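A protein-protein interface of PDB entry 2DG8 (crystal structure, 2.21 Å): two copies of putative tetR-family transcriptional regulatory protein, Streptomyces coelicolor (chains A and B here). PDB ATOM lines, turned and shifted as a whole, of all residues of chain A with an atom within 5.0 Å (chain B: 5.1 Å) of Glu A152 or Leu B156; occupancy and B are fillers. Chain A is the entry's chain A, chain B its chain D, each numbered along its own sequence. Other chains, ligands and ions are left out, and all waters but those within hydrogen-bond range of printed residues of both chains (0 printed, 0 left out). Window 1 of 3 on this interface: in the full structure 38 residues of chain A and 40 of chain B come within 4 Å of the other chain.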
ATOM      1  N   THR A 107     -17.090 -13.659   8.268  1.00  0.00           N
ATOM      2  CA  THR A 107     -18.229 -13.900   7.403  1.00  0.00           C
ATOM      3  C   THR A 107     -18.301 -15.398   7.104  1.00  0.00           C
ATOM      4  O   THR A 107     -19.353 -16.018   7.231  1.00  0.00           O
ATOM      5  CB  THR A 107     -18.104 -13.134   6.050  1.00  0.00           C
ATOM      6  OG1 THR A 107     -18.047 -11.727   6.292  1.00  0.00           O
ATOM      7  CG2 THR A 107     -19.291 -13.424   5.163  1.00  0.00           C
ATOM      8  N   TYR A 111     -21.173 -18.328   8.138  1.00  0.00           N
ATOM      9  CA  TYR A 111     -21.847 -19.151   7.135  1.00  0.00           C
ATOM     10  C   TYR A 111     -21.721 -20.648   7.426  1.00  0.00           C
ATOM     11  O   TYR A 111     -22.666 -21.403   7.204  1.00  0.00           O
ATOM     12  CB  TYR A 111     -21.292 -18.844   5.740  1.00  0.00           C
ATOM     13  CG  TYR A 111     -21.686 -17.489   5.209  1.00  0.00           C
ATOM     14  CD1 TYR A 111     -21.123 -16.983   4.041  1.00  0.00           C
ATOM     15  CD2 TYR A 111     -22.633 -16.709   5.874  1.00  0.00           C
ATOM     16  CE1 TYR A 111     -21.493 -15.734   3.549  1.00  0.00           C
ATOM     17  CE2 TYR A 111     -23.005 -15.472   5.395  1.00  0.00           C
ATOM     18  CZ  TYR A 111     -22.437 -14.987   4.237  1.00  0.00           C
ATOM     19  OH  TYR A 111     -22.817 -13.757   3.775  1.00  0.00           O
ATOM     20  N   LEU A 147     -29.885  -8.560  -6.548  1.00  0.00           N
ATOM     21  CA  LEU A 147     -28.630  -7.834  -6.400  1.00  0.00           C
ATOM     22  C   LEU A 147     -27.839  -8.270  -5.167  1.00  0.00           C
ATOM     23  O   LEU A 147     -26.611  -8.390  -5.225  1.00  0.00           O
ATOM     24  CB  LEU A 147     -28.902  -6.325  -6.346  1.00  0.00           C
ATOM     25  CG  LEU A 147     -27.687  -5.407  -6.243  1.00  0.00           C
ATOM     26  CD1 LEU A 147     -26.630  -5.799  -7.291  1.00  0.00           C
ATOM     27  CD2 LEU A 147     -28.144  -3.959  -6.429  1.00  0.00           C
ATOM     28  N   ASP A 148     -28.533  -8.515  -4.059  1.00  0.00           N
ATOM     29  CA  ASP A 148     -27.860  -8.946  -2.831  1.00  0.00           C
ATOM     30  C   ASP A 148     -27.154 -10.278  -3.065  1.00  0.00           C
ATOM     31  O   ASP A 148     -26.059 -10.503  -2.552  1.00  0.00           O
ATOM     32  CB  ASP A 148     -28.854  -9.104  -1.674  1.00  0.00           C
ATOM     33  CG  ASP A 148     -28.163  -9.111  -0.306  1.00  0.00           C
ATOM     34  OD1 ASP A 148     -28.672  -9.767   0.632  1.00  0.00           O
ATOM     35  OD2 ASP A 148     -27.109  -8.448  -0.167  1.00  0.00           O
ATOM     36  N   ALA A 149     -27.780 -11.169  -3.833  1.00  0.00           N
ATOM     37  CA  ALA A 149     -27.163 -12.458  -4.122  1.00  0.00           C
ATOM     38  C   ALA A 149     -25.951 -12.275  -5.037  1.00  0.00           C
ATOM     39  O   ALA A 149     -24.974 -13.023  -4.938  1.00  0.00           O
ATOM     40  CB  ALA A 149     -28.172 -13.399  -4.778  1.00  0.00           C
ATOM     41  N   LEU A 150     -26.020 -11.292  -5.936  1.00  0.00           N
ATOM     42  CA  LEU A 150     -24.905 -11.034  -6.848  1.00  0.00           C
ATOM     43  C   LEU A 150     -23.733 -10.485  -6.044  1.00  0.00           C
ATOM     44  O   LEU A 150     -22.594 -10.936  -6.198  1.00  0.00           O
ATOM     45  CB  LEU A 150     -25.298 -10.025  -7.941  1.00  0.00           C
ATOM     46  CG  LEU A 150     -24.199  -9.637  -8.939  1.00  0.00           C
ATOM     47  CD1 LEU A 150     -23.744 -10.883  -9.702  1.00  0.00           C
ATOM     48  CD2 LEU A 150     -24.715  -8.576  -9.916  1.00  0.00           C
ATOM     49  N   ILE A 151     -24.018  -9.505  -5.192  1.00  0.00           N
ATOM     50  CA  ILE A 151     -22.989  -8.894  -4.355  1.00  0.00           C
ATOM     51  C   ILE A 151     -22.283  -9.986  -3.553  1.00  0.00           C
ATOM     52  O   ILE A 151     -21.047 -10.001  -3.437  1.00  0.00           O
ATOM     53  CB  ILE A 151     -23.612  -7.844  -3.384  1.00  0.00           C
ATOM     54  CG1 ILE A 151     -24.059  -6.616  -4.178  1.00  0.00           C
ATOM     55  CG2 ILE A 151     -22.617  -7.454  -2.294  1.00  0.00           C
ATOM     56  CD1 ILE A 151     -24.773  -5.574  -3.351  1.00  0.00           C
ATOM     57  N   GLU A 152     -23.078 -10.903  -3.015  1.00  0.00           N
ATOM     58  CA  GLU A 152     -22.550 -12.009  -2.225  1.00  0.00           C
ATOM     59  C   GLU A 152     -21.570 -12.829  -3.062  1.00  0.00           C
ATOM     60  O   GLU A 152     -20.448 -13.095  -2.640  1.00  0.00           O
ATOM     61  CB  GLU A 152     -23.698 -12.908  -1.762  1.00  0.00           C
ATOM     62  CG  GLU A 152     -23.294 -13.980  -0.783  1.00  0.00           C
ATOM     63  CD  GLU A 152     -23.122 -13.433   0.622  1.00  0.00           C
ATOM     64  OE1 GLU A 152     -24.092 -12.847   1.154  1.00  0.00           O
ATOM     65  OE2 GLU A 152     -22.021 -13.588   1.189  1.00  0.00           O
ATOM     66  N   GLY A 153     -22.013 -13.221  -4.252  1.00  0.00           N
ATOM     67  CA  GLY A 153     -21.190 -14.022  -5.140  1.00  0.00           C
ATOM     68  C   GLY A 153     -19.954 -13.343  -5.711  1.00  0.00           C
ATOM     69  O   GLY A 153     -18.897 -13.968  -5.798  1.00  0.00           O
ATOM     70  N   LEU A 154     -20.080 -12.078  -6.110  1.00  0.00           N
ATOM     71  CA  LEU A 154     -18.949 -11.330  -6.662  1.00  0.00           C
ATOM     72  C   LEU A 154     -17.880 -11.134  -5.594  1.00  0.00           C
ATOM     73  O   LEU A 154     -16.691 -11.264  -5.859  1.00  0.00           O
ATOM     74  CB  LEU A 154     -19.403  -9.955  -7.191  1.00  0.00           C
ATOM     75  CG  LEU A 154     -20.206  -9.908  -8.504  1.00  0.00           C
ATOM     76  CD1 LEU A 154     -20.733  -8.491  -8.760  1.00  0.00           C
ATOM     77  CD2 LEU A 154     -19.327 -10.351  -9.659  1.00  0.00           C
ATOM     78  N   THR A 155     -18.319 -10.823  -4.383  1.00  0.00           N
ATOM     79  CA  THR A 155     -17.417 -10.607  -3.260  1.00  0.00           C
ATOM     80  C   THR A 155     -16.615 -11.872  -2.975  1.00  0.00           C
ATOM     81  O   THR A 155     -15.387 -11.841  -2.844  1.00  0.00           O
ATOM     82  CB  THR A 155     -18.220 -10.226  -1.998  1.00  0.00           C
ATOM     83  OG1 THR A 155     -18.925  -8.995  -2.235  1.00  0.00           O
ATOM     84  CG2 THR A 155     -17.304 -10.072  -0.803  1.00  0.00           C
ATOM     85  N   LEU A 156     -17.333 -12.985  -2.886  1.00  0.00           N
ATOM     86  CA  LEU A 156     -16.741 -14.274  -2.605  1.00  0.00           C
ATOM     87  C   LEU A 156     -15.748 -14.682  -3.679  1.00  0.00           C
ATOM     88  O   LEU A 156     -14.655 -15.145  -3.369  1.00  0.00           O
ATOM     89  CB  LEU A 156     -17.843 -15.328  -2.486  1.00  0.00           C
ATOM     90  CG  LEU A 156     -17.507 -16.719  -1.937  1.00  0.00           C
ATOM     91  CD1 LEU A 156     -16.768 -17.542  -2.986  1.00  0.00           C
ATOM     92  CD2 LEU A 156     -16.678 -16.573  -0.669  1.00  0.00           C
ATOM     93  N   GLN B 108     -18.593 -24.714   2.452  1.00  0.00           N
ATOM     94  CA  GLN B 108     -18.332 -23.659   3.431  1.00  0.00           C
ATOM     95  C   GLN B 108     -16.997 -23.866   4.133  1.00  0.00           C
ATOM     96  O   GLN B 108     -16.272 -22.910   4.376  1.00  0.00           O
ATOM     97  CB  GLN B 108     -19.469 -23.565   4.462  1.00  0.00           C
ATOM     98  CG  GLN B 108     -20.825 -23.192   3.862  1.00  0.00           C
ATOM     99  CD  GLN B 108     -20.769 -21.929   2.999  1.00  0.00           C
ATOM    100  OE1 GLN B 108     -20.382 -20.852   3.460  1.00  0.00           O
ATOM    101  NE2 GLN B 108     -21.161 -22.064   1.738  1.00  0.00           N
ATOM    102  N   ILE B 151     -24.440 -17.594  -9.569  1.00  0.00           N
ATOM    103  CA  ILE B 151     -24.777 -18.944  -9.132  1.00  0.00           C
ATOM    104  C   ILE B 151     -24.323 -19.140  -7.697  1.00  0.00           C
ATOM    105  O   ILE B 151     -25.057 -19.691  -6.865  1.00  0.00           O
ATOM    106  CB  ILE B 151     -24.101 -20.002 -10.011  1.00  0.00           C
ATOM    107  CG1 ILE B 151     -24.766 -20.010 -11.389  1.00  0.00           C
ATOM    108  CG2 ILE B 151     -24.192 -21.386  -9.345  1.00  0.00           C
ATOM    109  CD1 ILE B 151     -24.058 -20.880 -12.395  1.00  0.00           C
ATOM    110  N   GLU B 152     -23.113 -18.677  -7.407  1.00  0.00           N
ATOM    111  CA  GLU B 152     -22.547 -18.788  -6.067  1.00  0.00           C
ATOM    112  C   GLU B 152     -23.430 -18.058  -5.058  1.00  0.00           C
ATOM    113  O   GLU B 152     -23.884 -18.643  -4.079  1.00  0.00           O
ATOM    114  CB  GLU B 152     -21.139 -18.187  -6.047  1.00  0.00           C
ATOM    115  CG  GLU B 152     -20.335 -18.475  -4.790  1.00  0.00           C
ATOM    116  CD  GLU B 152     -19.795 -19.889  -4.765  1.00  0.00           C
ATOM    117  OE1 GLU B 152     -19.095 -20.280  -5.729  1.00  0.00           O
ATOM    118  OE2 GLU B 152     -20.071 -20.608  -3.780  1.00  0.00           O
ATOM    119  N   GLY B 153     -23.677 -16.775  -5.306  1.00  0.00           N
ATOM    120  CA  GLY B 153     -24.499 -15.994  -4.402  1.00  0.00           C
ATOM    121  C   GLY B 153     -25.915 -16.512  -4.202  1.00  0.00           C
ATOM    122  O   GLY B 153     -26.395 -16.580  -3.072  1.00  0.00           O
ATOM    123  N   LEU B 154     -26.600 -16.868  -5.285  1.00  0.00           N
ATOM    124  CA  LEU B 154     -27.968 -17.378  -5.157  1.00  0.00           C
ATOM    125  C   LEU B 154     -27.994 -18.669  -4.328  1.00  0.00           C
ATOM    126  O   LEU B 154     -28.852 -18.849  -3.466  1.00  0.00           O
ATOM    127  CB  LEU B 154     -28.572 -17.644  -6.544  1.00  0.00           C
ATOM    128  CG  LEU B 154     -28.842 -16.436  -7.444  1.00  0.00           C
ATOM    129  CD1 LEU B 154     -29.260 -16.906  -8.834  1.00  0.00           C
ATOM    130  CD2 LEU B 154     -29.933 -15.560  -6.815  1.00  0.00           C
ATOM    131  N   THR B 155     -27.055 -19.568  -4.602  1.00  0.00           N
ATOM    132  CA  THR B 155     -26.989 -20.831  -3.884  1.00  0.00           C
ATOM    133  C   THR B 155     -26.828 -20.604  -2.384  1.00  0.00           C
ATOM    134  O   THR B 155     -27.564 -21.173  -1.590  1.00  0.00           O
ATOM    135  CB  THR B 155     -25.826 -21.701  -4.404  1.00  0.00           C
ATOM    136  OG1 THR B 155     -26.067 -22.037  -5.775  1.00  0.00           O
ATOM    137  CG2 THR B 155     -25.716 -22.992  -3.596  1.00  0.00           C
ATOM    138  N   LEU B 156     -25.874 -19.758  -2.007  1.00  0.00           N
ATOM    139  CA  LEU B 156     -25.630 -19.449  -0.600  1.00  0.00           C
ATOM    140  C   LEU B 156     -26.852 -18.786   0.044  1.00  0.00           C
ATOM    141  O   LEU B 156     -27.248 -19.147   1.155  1.00  0.00           O
ATOM    142  CB  LEU B 156     -24.388 -18.549  -0.475  1.00  0.00           C
ATOM    143  CG  LEU B 156     -23.701 -18.287   0.879  1.00  0.00           C
ATOM    144  CD1 LEU B 156     -24.318 -17.091   1.577  1.00  0.00           C
ATOM    145  CD2 LEU B 156     -23.785 -19.533   1.748  1.00  0.00           C
ATOM    146  N   HIS B 157     -27.464 -17.829  -0.647  1.00  0.00           N
ATOM    147  CA  HIS B 157     -28.639 -17.171  -0.082  1.00  0.00           C
ATOM    148  C   HIS B 157     -29.835 -18.110   0.106  1.00  0.00           C
ATOM    149  O   HIS B 157     -30.590 -17.964   1.068  1.00  0.00           O
ATOM    150  CB  HIS B 157     -29.040 -15.958  -0.924  1.00  0.00           C
ATOM    151  CG  HIS B 157     -28.222 -14.740  -0.635  1.00  0.00           C
ATOM    152  ND1 HIS B 157     -28.546 -13.492  -1.122  1.00  0.00           N
ATOM    153  CD2 HIS B 157     -27.124 -14.568   0.137  1.00  0.00           C
ATOM    154  CE1 HIS B 157     -27.690 -12.602  -0.654  1.00  0.00           C
ATOM    155  NE2 HIS B 157     -26.816 -13.228   0.112  1.00  0.00           N
ATOM    156  N   ARG B 158     -30.015 -19.073  -0.796  1.00  0.00           N
ATOM    157  CA  ARG B 158     -31.114 -20.016  -0.636  1.00  0.00           C
ATOM    158  C   ARG B 158     -30.822 -20.941   0.542  1.00  0.00           C
ATOM    159  O   ARG B 158     -31.702 -21.213   1.356  1.00  0.00           O
ATOM    160  CB  ARG B 158     -31.320 -20.875  -1.892  1.00  0.00           C
ATOM    161  CG  ARG B 158     -31.916 -20.141  -3.075  1.00  0.00           C
ATOM    162  CD  ARG B 158     -32.621 -21.104  -4.025  1.00  0.00           C
ATOM    163  NE  ARG B 158     -33.955 -21.475  -3.540  1.00  0.00           N
ATOM    164  CZ  ARG B 158     -34.344 -22.717  -3.260  1.00  0.00           C
ATOM    165  NH1 ARG B 158     -35.582 -22.946  -2.828  1.00  0.00           N
ATOM    166  NH2 ARG B 158     -33.504 -23.729  -3.411  1.00  0.00           N
ATOM    167  N   ALA B 159     -29.578 -21.404   0.637  1.00  0.00           N
ATOM    168  CA  ALA B 159     -29.168 -22.331   1.697  1.00  0.00           C
ATOM    169  C   ALA B 159     -29.165 -21.794   3.128  1.00  0.00           C
ATOM    170  O   ALA B 159     -29.533 -22.511   4.055  1.00  0.00           O
ATOM    171  CB  ALA B 159     -27.784 -22.913   1.373  1.00  0.00           C
ATOM    172  N   LEU B 160     -28.751 -20.549   3.313  1.00  0.00           N
ATOM    173  CA  LEU B 160     -28.681 -19.979   4.656  1.00  0.00           C
ATOM    174  C   LEU B 160     -29.860 -19.097   5.046  1.00  0.00           C
ATOM    175  O   LEU B 160     -29.783 -18.316   6.000  1.00  0.00           O
ATOM    176  CB  LEU B 160     -27.377 -19.197   4.815  1.00  0.00           C
ATOM    177  CG  LEU B 160     -26.101 -20.026   4.663  1.00  0.00           C
ATOM    178  CD1 LEU B 160     -24.900 -19.165   5.009  1.00  0.00           C
ATOM    179  CD2 LEU B 160     -26.163 -21.246   5.577  1.00  0.00           C
ATOM    180  N   ALA B 161     -30.956 -19.219   4.311  1.00  0.00           N
ATOM    181  CA  ALA B 161     -32.142 -18.431   4.609  1.00  0.00           C
ATOM    182  C   ALA B 161     -33.077 -19.300   5.423  1.00  0.00           C
ATOM    183  O   ALA B 161     -32.905 -20.517   5.482  1.00  0.00           O
ATOM    184  CB  ALA B 161     -32.827 -18.003   3.319  1.00  0.00           C
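OE1 of Glu A152 lies within hydrogen-bond range of NE2 of His B157, at 2.9 Å.
OH of Tyr A111 lies within hydrogen-bond range of OE2 of Glu A152 (2.7 Å).
OE1 of Gln B108 touches CB of Tyr A111, 3.2 Å away. Tyr A111 touches Leu B156. Tyr A111 touches Leu B160. His B157 touches Asp A148 (CE1 to OD1, 3.3 Å). Ala A149 touches Gly B153. Ala A149 touches Leu B154 (CB to CD2, 3.5 Å). Ala A149 touches His B157 (CA to ND1, 3.5 Å). Leu B156 touches Glu A152. Gly B153 touches Gly A153 (N to CA, 3.7 Å).
Glu A152 touches just these residues of chain B: Leu B156 (3.97 Å) and His B157 (2.9 Å). Of the printed residues of chain A, Leu B156 touches Tyr A111 (3.7 Å) and Glu A152 (3.97 Å). Printed residues of chain A within 4 Å of Gln B108: Tyr A111. Of the printed residues of chain B, Gly A153 touches Gly B153. Of the printed residues of chain A, His B157 touches Asp A148, Ala A149 and Glu A152. Leu A147 touches none of the printed residues of chain B. The nearest residue of chain B that does not touch Glu A152 is Gly B153 (4.1 Å).
Of the 12 printed residues of chain B, 6 touch a printed residue of chain A. Along chain B the printed residues that touch a printed residue of chain A span positions 108 to 160. Of the 12 printed residues of chain A, 5 touch a printed residue of chain B. Among the printed residues, 10 pairs touch across the chains. Among the printed residues, no Asp or Glu carboxylate lies within 4 Å of a Lys or Arg side-chain nitrogen of the other chain.
Glu A152 touches Leu B156, but with the chains exchanged Leu A156 does not touch Glu B152 (4.1 Å). Gly A153 touches its own counterpart, Gly B153. Of the 10 pairs that touch across the chains among the printed residues, 1 has its exchanged pair printed and touching as well.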
